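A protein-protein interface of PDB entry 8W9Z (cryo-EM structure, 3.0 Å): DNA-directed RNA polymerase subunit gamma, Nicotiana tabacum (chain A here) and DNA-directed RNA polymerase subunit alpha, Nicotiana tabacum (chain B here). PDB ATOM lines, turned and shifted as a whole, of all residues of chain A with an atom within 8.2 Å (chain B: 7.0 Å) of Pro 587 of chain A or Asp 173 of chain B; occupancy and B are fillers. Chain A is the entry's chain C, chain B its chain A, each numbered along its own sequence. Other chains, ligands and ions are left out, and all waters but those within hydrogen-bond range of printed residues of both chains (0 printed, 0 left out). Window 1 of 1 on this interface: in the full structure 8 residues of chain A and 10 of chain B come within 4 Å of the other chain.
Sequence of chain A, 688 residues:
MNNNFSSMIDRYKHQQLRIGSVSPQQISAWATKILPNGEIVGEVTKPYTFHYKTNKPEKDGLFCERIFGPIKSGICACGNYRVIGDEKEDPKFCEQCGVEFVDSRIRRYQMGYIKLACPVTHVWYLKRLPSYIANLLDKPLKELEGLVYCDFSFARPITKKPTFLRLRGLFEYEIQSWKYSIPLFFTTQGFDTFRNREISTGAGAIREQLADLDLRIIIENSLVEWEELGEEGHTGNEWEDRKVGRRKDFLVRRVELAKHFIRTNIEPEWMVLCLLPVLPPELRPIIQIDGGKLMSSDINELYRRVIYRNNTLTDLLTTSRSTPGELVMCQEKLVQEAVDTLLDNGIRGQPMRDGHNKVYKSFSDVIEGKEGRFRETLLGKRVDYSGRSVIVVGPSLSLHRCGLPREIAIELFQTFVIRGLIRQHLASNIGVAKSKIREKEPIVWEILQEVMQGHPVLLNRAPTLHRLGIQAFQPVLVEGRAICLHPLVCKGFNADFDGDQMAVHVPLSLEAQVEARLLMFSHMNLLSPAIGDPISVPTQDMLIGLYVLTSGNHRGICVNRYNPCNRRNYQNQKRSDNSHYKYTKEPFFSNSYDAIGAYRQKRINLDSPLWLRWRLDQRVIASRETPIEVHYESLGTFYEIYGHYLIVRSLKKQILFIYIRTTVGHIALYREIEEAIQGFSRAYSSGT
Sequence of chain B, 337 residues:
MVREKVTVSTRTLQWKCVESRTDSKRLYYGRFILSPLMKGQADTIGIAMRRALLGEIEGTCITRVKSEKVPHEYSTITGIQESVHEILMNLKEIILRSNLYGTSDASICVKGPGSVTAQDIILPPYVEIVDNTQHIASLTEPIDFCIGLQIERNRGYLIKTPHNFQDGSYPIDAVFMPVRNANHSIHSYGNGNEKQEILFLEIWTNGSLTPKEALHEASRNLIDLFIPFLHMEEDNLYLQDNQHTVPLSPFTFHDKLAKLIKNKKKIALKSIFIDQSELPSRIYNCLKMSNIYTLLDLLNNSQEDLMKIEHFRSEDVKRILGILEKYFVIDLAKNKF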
ATOM      1  N   THR A 584     -15.030   9.242 -24.736  1.00  0.00           N
ATOM      2  CA  THR A 584     -15.886   9.130 -23.562  1.00  0.00           C
ATOM      3  C   THR A 584     -15.661   7.804 -22.842  1.00  0.00           C
ATOM      4  O   THR A 584     -15.176   6.840 -23.435  1.00  0.00           O
ATOM      5  CB  THR A 584     -17.377   9.255 -23.936  1.00  0.00           C
ATOM      6  OG1 THR A 584     -18.182   9.103 -22.760  1.00  0.00           O
ATOM      7  CG2 THR A 584     -17.764   8.191 -24.951  1.00  0.00           C
ATOM      8  N   LYS A 585     -16.014   7.764 -21.561  1.00  0.00           N
ATOM      9  CA  LYS A 585     -15.864   6.556 -20.761  1.00  0.00           C
ATOM     10  C   LYS A 585     -17.068   5.643 -20.989  1.00  0.00           C
ATOM     11  O   LYS A 585     -17.884   5.858 -21.888  1.00  0.00           O
ATOM     12  CB  LYS A 585     -15.687   6.912 -19.288  1.00  0.00           C
ATOM     13  CG  LYS A 585     -14.475   7.781 -19.001  1.00  0.00           C
ATOM     14  CD  LYS A 585     -13.188   7.102 -19.439  1.00  0.00           C
ATOM     15  CE  LYS A 585     -12.952   5.812 -18.672  1.00  0.00           C
ATOM     16  NZ  LYS A 585     -11.696   5.137 -19.102  1.00  0.00           N
ATOM     17  N   GLU A 586     -17.184   4.603 -20.168  1.00  0.00           N
ATOM     18  CA  GLU A 586     -18.304   3.687 -20.280  1.00  0.00           C
ATOM     19  C   GLU A 586     -19.606   4.398 -19.916  1.00  0.00           C
ATOM     20  O   GLU A 586     -19.601   5.350 -19.132  1.00  0.00           O
ATOM     21  CB  GLU A 586     -18.094   2.476 -19.375  1.00  0.00           C
ATOM     22  CG  GLU A 586     -16.821   1.696 -19.670  1.00  0.00           C
ATOM     23  CD  GLU A 586     -16.806   1.098 -21.064  1.00  0.00           C
ATOM     24  OE1 GLU A 586     -17.894   0.809 -21.606  1.00  0.00           O
ATOM     25  OE2 GLU A 586     -15.702   0.914 -21.620  1.00  0.00           O
ATOM     26  N   PRO A 587     -20.731   3.966 -20.485  1.00  0.00           N
ATOM     27  CA  PRO A 587     -22.005   4.636 -20.199  1.00  0.00           C
ATOM     28  C   PRO A 587     -22.347   4.592 -18.717  1.00  0.00           C
ATOM     29  O   PRO A 587     -21.894   3.724 -17.967  1.00  0.00           O
ATOM     30  CB  PRO A 587     -23.022   3.843 -21.032  1.00  0.00           C
ATOM     31  CG  PRO A 587     -22.357   2.533 -21.312  1.00  0.00           C
ATOM     32  CD  PRO A 587     -20.899   2.848 -21.428  1.00  0.00           C
ATOM     33  N   PHE A 588     -23.160   5.558 -18.300  1.00  0.00           N
ATOM     34  CA  PHE A 588     -23.534   5.694 -16.897  1.00  0.00           C
ATOM     35  C   PHE A 588     -24.406   4.514 -16.489  1.00  0.00           C
ATOM     36  O   PHE A 588     -25.586   4.446 -16.850  1.00  0.00           O
ATOM     37  CB  PHE A 588     -24.260   7.017 -16.675  1.00  0.00           C
ATOM     38  CG  PHE A 588     -23.466   8.224 -17.091  1.00  0.00           C
ATOM     39  CD1 PHE A 588     -23.553   8.717 -18.382  1.00  0.00           C
ATOM     40  CD2 PHE A 588     -22.633   8.866 -16.190  1.00  0.00           C
ATOM     41  CE1 PHE A 588     -22.822   9.827 -18.768  1.00  0.00           C
ATOM     42  CE2 PHE A 588     -21.900   9.975 -16.569  1.00  0.00           C
ATOM     43  CZ  PHE A 588     -21.994  10.456 -17.859  1.00  0.00           C
ATOM     44  N   PHE A 589     -23.828   3.582 -15.736  1.00  0.00           N
ATOM     45  CA  PHE A 589     -24.558   2.412 -15.266  1.00  0.00           C
ATOM     46  C   PHE A 589     -25.461   2.808 -14.104  1.00  0.00           C
ATOM     47  O   PHE A 589     -24.978   3.265 -13.063  1.00  0.00           O
ATOM     48  CB  PHE A 589     -23.587   1.311 -14.849  1.00  0.00           C
ATOM     49  CG  PHE A 589     -22.872   0.667 -16.002  1.00  0.00           C
ATOM     50  CD1 PHE A 589     -23.493   0.534 -17.231  1.00  0.00           C
ATOM     51  CD2 PHE A 589     -21.578   0.199 -15.858  1.00  0.00           C
ATOM     52  CE1 PHE A 589     -22.839  -0.058 -18.294  1.00  0.00           C
ATOM     53  CE2 PHE A 589     -20.918  -0.393 -16.918  1.00  0.00           C
ATOM     54  CZ  PHE A 589     -21.550  -0.522 -18.137  1.00  0.00           C
ATOM     55  N   SER A 590     -26.771   2.637 -14.285  1.00  0.00           N
ATOM     56  CA  SER A 590     -27.719   3.029 -13.248  1.00  0.00           C
ATOM     57  C   SER A 590     -27.629   2.126 -12.025  1.00  0.00           C
ATOM     58  O   SER A 590     -27.885   2.579 -10.904  1.00  0.00           O
ATOM     59  CB  SER A 590     -29.142   3.021 -13.810  1.00  0.00           C
ATOM     60  OG  SER A 590     -29.256   3.900 -14.916  1.00  0.00           O
ATOM     61  N   ASN A 591     -27.271   0.858 -12.213  1.00  0.00           N
ATOM     62  CA  ASN A 591     -27.176  -0.096 -11.120  1.00  0.00           C
ATOM     63  C   ASN A 591     -25.896  -0.908 -11.255  1.00  0.00           C
ATOM     64  O   ASN A 591     -25.368  -1.087 -12.356  1.00  0.00           O
ATOM     65  CB  ASN A 591     -28.388  -1.039 -11.090  1.00  0.00           C
ATOM     66  CG  ASN A 591     -29.702  -0.295 -10.959  1.00  0.00           C
ATOM     67  OD1 ASN A 591     -30.573  -0.395 -11.822  1.00  0.00           O
ATOM     68  ND2 ASN A 591     -29.850   0.458  -9.875  1.00  0.00           N
ATOM     69  N   ALA A 595     -23.657  -3.293 -14.315  1.00  0.00           N
ATOM     70  CA  ALA A 595     -22.210  -3.298 -14.499  1.00  0.00           C
ATOM     71  C   ALA A 595     -21.653  -4.716 -14.449  1.00  0.00           C
ATOM     72  O   ALA A 595     -20.828  -5.099 -15.289  1.00  0.00           O
ATOM     73  CB  ALA A 595     -21.542  -2.423 -13.441  1.00  0.00           C
ATOM     74  N   ALA A 598     -22.630  -6.522 -17.625  1.00  0.00           N
ATOM     75  CA  ALA A 598     -21.797  -6.133 -18.756  1.00  0.00           C
ATOM     76  C   ALA A 598     -20.395  -6.714 -18.641  1.00  0.00           C
ATOM     77  O   ALA A 598     -19.771  -7.028 -19.661  1.00  0.00           O
ATOM     78  CB  ALA A 598     -21.735  -4.609 -18.864  1.00  0.00           C
ATOM     79  N   ARG A 603     -18.020  -7.147 -22.246  1.00  0.00           N
ATOM     80  CA  ARG A 603     -18.069  -5.875 -22.952  1.00  0.00           C
ATOM     81  C   ARG A 603     -17.222  -4.795 -22.299  1.00  0.00           C
ATOM     82  O   ARG A 603     -16.852  -3.831 -22.975  1.00  0.00           O
ATOM     83  CB  ARG A 603     -19.517  -5.378 -23.066  1.00  0.00           C
ATOM     84  CG  ARG A 603     -20.420  -6.305 -23.863  1.00  0.00           C
ATOM     85  CD  ARG A 603     -21.789  -5.690 -24.098  1.00  0.00           C
ATOM     86  NE  ARG A 603     -22.647  -6.565 -24.891  1.00  0.00           N
ATOM     87  CZ  ARG A 603     -22.667  -6.586 -26.220  1.00  0.00           C
ATOM     88  NH1 ARG A 603     -21.874  -5.778 -26.911  1.00  0.00           N
ATOM     89  NH2 ARG A 603     -23.481  -7.416 -26.860  1.00  0.00           N
ATOM     90  N   ILE A 604     -16.909  -4.934 -21.014  1.00  0.00           N
ATOM     91  CA  ILE A 604     -15.997  -4.042 -20.313  1.00  0.00           C
ATOM     92  C   ILE A 604     -14.991  -4.893 -19.553  1.00  0.00           C
ATOM     93  O   ILE A 604     -15.299  -6.002 -19.106  1.00  0.00           O
ATOM     94  CB  ILE A 604     -16.735  -3.081 -19.354  1.00  0.00           C
ATOM     95  CG1 ILE A 604     -17.519  -3.868 -18.303  1.00  0.00           C
ATOM     96  CG2 ILE A 604     -17.661  -2.158 -20.129  1.00  0.00           C
ATOM     97  CD1 ILE A 604     -18.264  -2.997 -17.318  1.00  0.00           C
ATOM     98  N   PRO A 609     -12.526   1.860 -16.303  1.00  0.00           N
ATOM     99  CA  PRO A 609     -13.319   2.741 -15.440  1.00  0.00           C
ATOM    100  C   PRO A 609     -14.729   2.925 -15.977  1.00  0.00           C
ATOM    101  O   PRO A 609     -14.984   2.815 -17.179  1.00  0.00           O
ATOM    102  CB  PRO A 609     -12.541   4.063 -15.463  1.00  0.00           C
ATOM    103  CG  PRO A 609     -11.178   3.710 -15.982  1.00  0.00           C
ATOM    104  CD  PRO A 609     -11.395   2.569 -16.920  1.00  0.00           C
ATOM    105  N   LEU A 610     -15.652   3.212 -15.063  1.00  0.00           N
ATOM    106  CA  LEU A 610     -17.046   3.422 -15.422  1.00  0.00           C
ATOM    107  C   LEU A 610     -17.677   4.374 -14.419  1.00  0.00           C
ATOM    108  O   LEU A 610     -17.121   4.649 -13.353  1.00  0.00           O
ATOM    109  CB  LEU A 610     -17.812   2.093 -15.489  1.00  0.00           C
ATOM    110  CG  LEU A 610     -17.701   1.116 -14.314  1.00  0.00           C
ATOM    111  CD1 LEU A 610     -18.682   1.446 -13.196  1.00  0.00           C
ATOM    112  CD2 LEU A 610     -17.900  -0.312 -14.792  1.00  0.00           C
ATOM    113  N   TRP A 611     -18.857   4.876 -14.774  1.00  0.00           N
ATOM    114  CA  TRP A 611     -19.624   5.778 -13.925  1.00  0.00           C
ATOM    115  C   TRP A 611     -20.839   5.035 -13.390  1.00  0.00           C
ATOM    116  O   TRP A 611     -21.652   4.527 -14.168  1.00  0.00           O
ATOM    117  CB  TRP A 611     -20.055   7.026 -14.697  1.00  0.00           C
ATOM    118  CG  TRP A 611     -18.931   7.958 -15.019  1.00  0.00           C
ATOM    119  CD1 TRP A 611     -18.246   8.043 -16.195  1.00  0.00           C
ATOM    120  CD2 TRP A 611     -18.362   8.947 -14.153  1.00  0.00           C
ATOM    121  NE1 TRP A 611     -17.285   9.020 -16.113  1.00  0.00           N
ATOM    122  CE2 TRP A 611     -17.337   9.590 -14.869  1.00  0.00           C
ATOM    123  CE3 TRP A 611     -18.621   9.348 -12.839  1.00  0.00           C
ATOM    124  CZ2 TRP A 611     -16.570  10.612 -14.317  1.00  0.00           C
ATOM    125  CZ3 TRP A 611     -17.860  10.362 -12.294  1.00  0.00           C
ATOM    126  CH2 TRP A 611     -16.848  10.982 -13.032  1.00  0.00           C
ATOM    127  N   LEU A 612     -20.958   4.974 -12.067  1.00  0.00           N
ATOM    128  CA  LEU A 612     -22.064   4.297 -11.402  1.00  0.00           C
ATOM    129  C   LEU A 612     -22.920   5.334 -10.690  1.00  0.00           C
ATOM    130  O   LEU A 612     -22.421   6.079  -9.840  1.00  0.00           O
ATOM    131  CB  LEU A 612     -21.551   3.253 -10.410  1.00  0.00           C
ATOM    132  CG  LEU A 612     -22.625   2.427  -9.704  1.00  0.00           C
ATOM    133  CD1 LEU A 612     -23.383   1.566 -10.702  1.00  0.00           C
ATOM    134  CD2 LEU A 612     -22.014   1.571  -8.609  1.00  0.00           C
ATOM    135  N   ARG A 613     -24.203   5.379 -11.039  1.00  0.00           N
ATOM    136  CA  ARG A 613     -25.129   6.310 -10.409  1.00  0.00           C
ATOM    137  C   ARG A 613     -25.347   5.918  -8.953  1.00  0.00           C
ATOM    138  O   ARG A 613     -25.840   4.823  -8.665  1.00  0.00           O
ATOM    139  CB  ARG A 613     -26.453   6.325 -11.167  1.00  0.00           C
ATOM    140  CG  ARG A 613     -27.519   7.207 -10.544  1.00  0.00           C
ATOM    141  CD  ARG A 613     -28.811   7.143 -11.340  1.00  0.00           C
ATOM    142  NE  ARG A 613     -29.865   7.954 -10.739  1.00  0.00           N
ATOM    143  CZ  ARG A 613     -30.084   9.231 -11.034  1.00  0.00           C
ATOM    144  NH1 ARG A 613     -29.322   9.846 -11.926  1.00  0.00           N
ATOM    145  NH2 ARG A 613     -31.066   9.892 -10.437  1.00  0.00           N
ATOM    146  N   TYR A 659     -22.594  10.662  -9.142  1.00  0.00           N
ATOM    147  CA  TYR A 659     -21.980   9.604  -9.929  1.00  0.00           C
ATOM    148  C   TYR A 659     -20.602   9.289  -9.369  1.00  0.00           C
ATOM    149  O   TYR A 659     -19.856  10.196  -8.991  1.00  0.00           O
ATOM    150  CB  TYR A 659     -21.869   9.999 -11.403  1.00  0.00           C
ATOM    151  CG  TYR A 659     -23.200  10.157 -12.101  1.00  0.00           C
ATOM    152  CD1 TYR A 659     -23.813   9.075 -12.716  1.00  0.00           C
ATOM    153  CD2 TYR A 659     -23.840  11.387 -12.148  1.00  0.00           C
ATOM    154  CE1 TYR A 659     -25.028   9.213 -13.358  1.00  0.00           C
ATOM    155  CE2 TYR A 659     -25.055  11.535 -12.788  1.00  0.00           C
ATOM    156  CZ  TYR A 659     -25.645  10.445 -13.391  1.00  0.00           C
ATOM    157  OH  TYR A 659     -26.856  10.587 -14.029  1.00  0.00           O
ATOM    158  N   CYS B  61     -35.669  -3.139 -27.524  1.00  0.00           N
ATOM    159  CA  CYS B  61     -35.477  -1.928 -26.742  1.00  0.00           C
ATOM    160  C   CYS B  61     -35.492  -0.732 -27.685  1.00  0.00           C
ATOM    161  O   CYS B  61     -35.717  -0.868 -28.891  1.00  0.00           O
ATOM    162  CB  CYS B  61     -34.177  -1.988 -25.934  1.00  0.00           C
ATOM    163  SG  CYS B  61     -32.672  -1.806 -26.916  1.00  0.00           S
ATOM    164  N   ILE B  62     -35.251   0.447 -27.124  1.00  0.00           N
ATOM    165  CA  ILE B  62     -35.282   1.702 -27.866  1.00  0.00           C
ATOM    166  C   ILE B  62     -33.857   2.055 -28.270  1.00  0.00           C
ATOM    167  O   ILE B  62     -32.971   2.170 -27.414  1.00  0.00           O
ATOM    168  CB  ILE B  62     -35.915   2.827 -27.035  1.00  0.00           C
ATOM    169  CG1 ILE B  62     -37.239   2.354 -26.431  1.00  0.00           C
ATOM    170  CG2 ILE B  62     -36.130   4.063 -27.890  1.00  0.00           C
ATOM    171  CD1 ILE B  62     -37.847   3.332 -25.458  1.00  0.00           C
ATOM    172  N   THR B  63     -33.634   2.227 -29.572  1.00  0.00           N
ATOM    173  CA  THR B  63     -32.303   2.530 -30.089  1.00  0.00           C
ATOM    174  C   THR B  63     -32.088   4.033 -30.254  1.00  0.00           C
ATOM    175  O   THR B  63     -31.173   4.606 -29.654  1.00  0.00           O
ATOM    176  CB  THR B  63     -32.080   1.807 -31.421  1.00  0.00           C
ATOM    177  OG1 THR B  63     -33.100   2.187 -32.352  1.00  0.00           O
ATOM    178  CG2 THR B  63     -32.119   0.301 -31.220  1.00  0.00           C
ATOM    179  N   MET B  89     -32.073   8.331 -20.014  1.00  0.00           N
ATOM    180  CA  MET B  89     -31.872   7.215 -19.096  1.00  0.00           C
ATOM    181  C   MET B  89     -33.192   6.576 -18.684  1.00  0.00           C
ATOM    182  O   MET B  89     -33.233   5.376 -18.391  1.00  0.00           O
ATOM    183  CB  MET B  89     -31.099   7.682 -17.863  1.00  0.00           C
ATOM    184  CG  MET B  89     -29.632   7.979 -18.130  1.00  0.00           C
ATOM    185  SD  MET B  89     -28.728   6.511 -18.657  1.00  0.00           S
ATOM    186  CE  MET B  89     -27.113   7.203 -19.002  1.00  0.00           C
ATOM    187  N   LYS B  92     -34.277   4.428 -21.841  1.00  0.00           N
ATOM    188  CA  LYS B  92     -33.505   3.208 -22.056  1.00  0.00           C
ATOM    189  C   LYS B  92     -33.905   2.089 -21.103  1.00  0.00           C
ATOM    190  O   LYS B  92     -33.556   0.930 -21.351  1.00  0.00           O
ATOM    191  CB  LYS B  92     -32.008   3.489 -21.921  1.00  0.00           C
ATOM    192  CG  LYS B  92     -31.529   3.657 -20.492  1.00  0.00           C
ATOM    193  CD  LYS B  92     -30.012   3.701 -20.427  1.00  0.00           C
ATOM    194  CE  LYS B  92     -29.400   2.421 -20.975  1.00  0.00           C
ATOM    195  NZ  LYS B  92     -29.846   1.223 -20.212  1.00  0.00           N
ATOM    196  N   LEU B 158     -26.412  -3.350 -30.233  1.00  0.00           N
ATOM    197  CA  LEU B 158     -26.283  -2.565 -31.458  1.00  0.00           C
ATOM    198  C   LEU B 158     -24.825  -2.136 -31.583  1.00  0.00           C
ATOM    199  O   LEU B 158     -24.405  -1.140 -30.988  1.00  0.00           O
ATOM    200  CB  LEU B 158     -27.223  -1.364 -31.439  1.00  0.00           C
ATOM    201  N   TYR B 170     -30.901  11.185 -31.266  1.00  0.00           N
ATOM    202  CA  TYR B 170     -29.898  10.918 -30.240  1.00  0.00           C
ATOM    203  C   TYR B 170     -29.830   9.421 -29.975  1.00  0.00           C
ATOM    204  O   TYR B 170     -30.716   8.869 -29.305  1.00  0.00           O
ATOM    205  CB  TYR B 170     -30.227  11.677 -28.951  1.00  0.00           C
ATOM    206  CG  TYR B 170     -30.160  13.182 -29.088  1.00  0.00           C
ATOM    207  CD1 TYR B 170     -29.387  13.776 -30.077  1.00  0.00           C
ATOM    208  CD2 TYR B 170     -30.869  14.009 -28.226  1.00  0.00           C
ATOM    209  CE1 TYR B 170     -29.324  15.150 -30.206  1.00  0.00           C
ATOM    210  CE2 TYR B 170     -30.811  15.384 -28.347  1.00  0.00           C
ATOM    211  CZ  TYR B 170     -30.038  15.949 -29.338  1.00  0.00           C
ATOM    212  OH  TYR B 170     -29.977  17.318 -29.462  1.00  0.00           O
ATOM    213  N   PRO B 171     -28.816   8.720 -30.482  1.00  0.00           N
ATOM    214  CA  PRO B 171     -28.744   7.270 -30.264  1.00  0.00           C
ATOM    215  C   PRO B 171     -28.532   6.932 -28.796  1.00  0.00           C
ATOM    216  O   PRO B 171     -27.789   7.610 -28.083  1.00  0.00           O
ATOM    217  CB  PRO B 171     -27.541   6.843 -31.114  1.00  0.00           C
ATOM    218  CG  PRO B 171     -27.349   7.953 -32.101  1.00  0.00           C
ATOM    219  CD  PRO B 171     -27.754   9.198 -31.378  1.00  0.00           C
ATOM    220  N   ILE B 172     -29.196   5.869 -28.352  1.00  0.00           N
ATOM    221  CA  ILE B 172     -29.092   5.377 -26.984  1.00  0.00           C
ATOM    222  C   ILE B 172     -28.370   4.038 -27.016  1.00  0.00           C
ATOM    223  O   ILE B 172     -28.822   3.095 -27.679  1.00  0.00           O
ATOM    224  CB  ILE B 172     -30.472   5.239 -26.321  1.00  0.00           C
ATOM    225  CG1 ILE B 172     -31.105   6.613 -26.109  1.00  0.00           C
ATOM    226  CG2 ILE B 172     -30.353   4.494 -25.003  1.00  0.00           C
ATOM    227  CD1 ILE B 172     -32.410   6.566 -25.349  1.00  0.00           C
ATOM    228  N   ASP B 173     -27.247   3.954 -26.303  1.00  0.00           N
ATOM    229  CA  ASP B 173     -26.477   2.715 -26.204  1.00  0.00           C
ATOM    230  C   ASP B 173     -27.097   1.847 -25.112  1.00  0.00           C
ATOM    231  O   ASP B 173     -26.614   1.761 -23.980  1.00  0.00           O
ATOM    232  CB  ASP B 173     -25.008   3.015 -25.928  1.00  0.00           C
ATOM    233  CG  ASP B 173     -24.817   4.043 -24.829  1.00  0.00           C
ATOM    234  OD1 ASP B 173     -25.831   4.575 -24.327  1.00  0.00           O
ATOM    235  OD2 ASP B 173     -23.655   4.320 -24.468  1.00  0.00           O
ATOM    236  N   ALA B 174     -28.194   1.187 -25.471  1.00  0.00           N
ATOM    237  CA  ALA B 174     -28.952   0.353 -24.548  1.00  0.00           C
ATOM    238  C   ALA B 174     -28.776  -1.113 -24.913  1.00  0.00           C
ATOM    239  O   ALA B 174     -28.988  -1.500 -26.068  1.00  0.00           O
ATOM    240  CB  ALA B 174     -30.436   0.727 -24.566  1.00  0.00           C
ATOM    241  N   VAL B 175     -28.387  -1.920 -23.931  1.00  0.00           N
ATOM    242  CA  VAL B 175     -28.258  -3.359 -24.122  1.00  0.00           C
ATOM    243  C   VAL B 175     -29.632  -4.003 -24.003  1.00  0.00           C
ATOM    244  O   VAL B 175     -30.489  -3.557 -23.230  1.00  0.00           O
ATOM    245  CB  VAL B 175     -27.256  -3.950 -23.108  1.00  0.00           C
ATOM    246  CG1 VAL B 175     -27.762  -3.776 -21.682  1.00  0.00           C
ATOM    247  CG2 VAL B 175     -26.972  -5.416 -23.414  1.00  0.00           C
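Asp 173 of chain B touches Pro 587 of chain A. Phe 588 of chain A touches Met 89 of chain B.
Of the 18 printed residues of chain A, 2 touch a printed residue of chain B. Printed residues of chain A that touch a printed residue of chain B: Pro 587 and Phe 588. Hydrophobic or aromatic side chains of chain A within 4 Å of the printed part of chain B: Pro 587 and Phe 588. Along chain A the printed residues that touch a printed residue of chain B span positions 587 to 588. Hydrophobic or aromatic side chains of chain B that line the printed part of chain A: Met 89. Along chain B the printed residues that touch a printed residue of chain A span positions 89 to 173.
Pro 587 of chain A touches one residue of chain B. Of the printed residues of chain B, Phe 588 of chain A touches Met 89. Pro 609 of chain A touches none of the printed residues of chain B. Of the printed residues of chain A, Met 89 of chain B touches Phe 588 (3.7 Å). Leu 158 of chain B touches none of the printed residues of chain A. Printed residues of chain A within 4 Å of Asp 173 of chain B: Pro 587 (3.5 Å). The nearest residue of chain B that does not touch Pro 587 of chain A is Met 89 of chain B (5.4 Å). The nearest residue of chain A that does not touch Asp 173 of chain B is Glu 586 of chain A (6.1 Å). The nearest printed residue of chain A that does not touch Met 89 of chain B is Ser 590 of chain A (4.6 Å).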
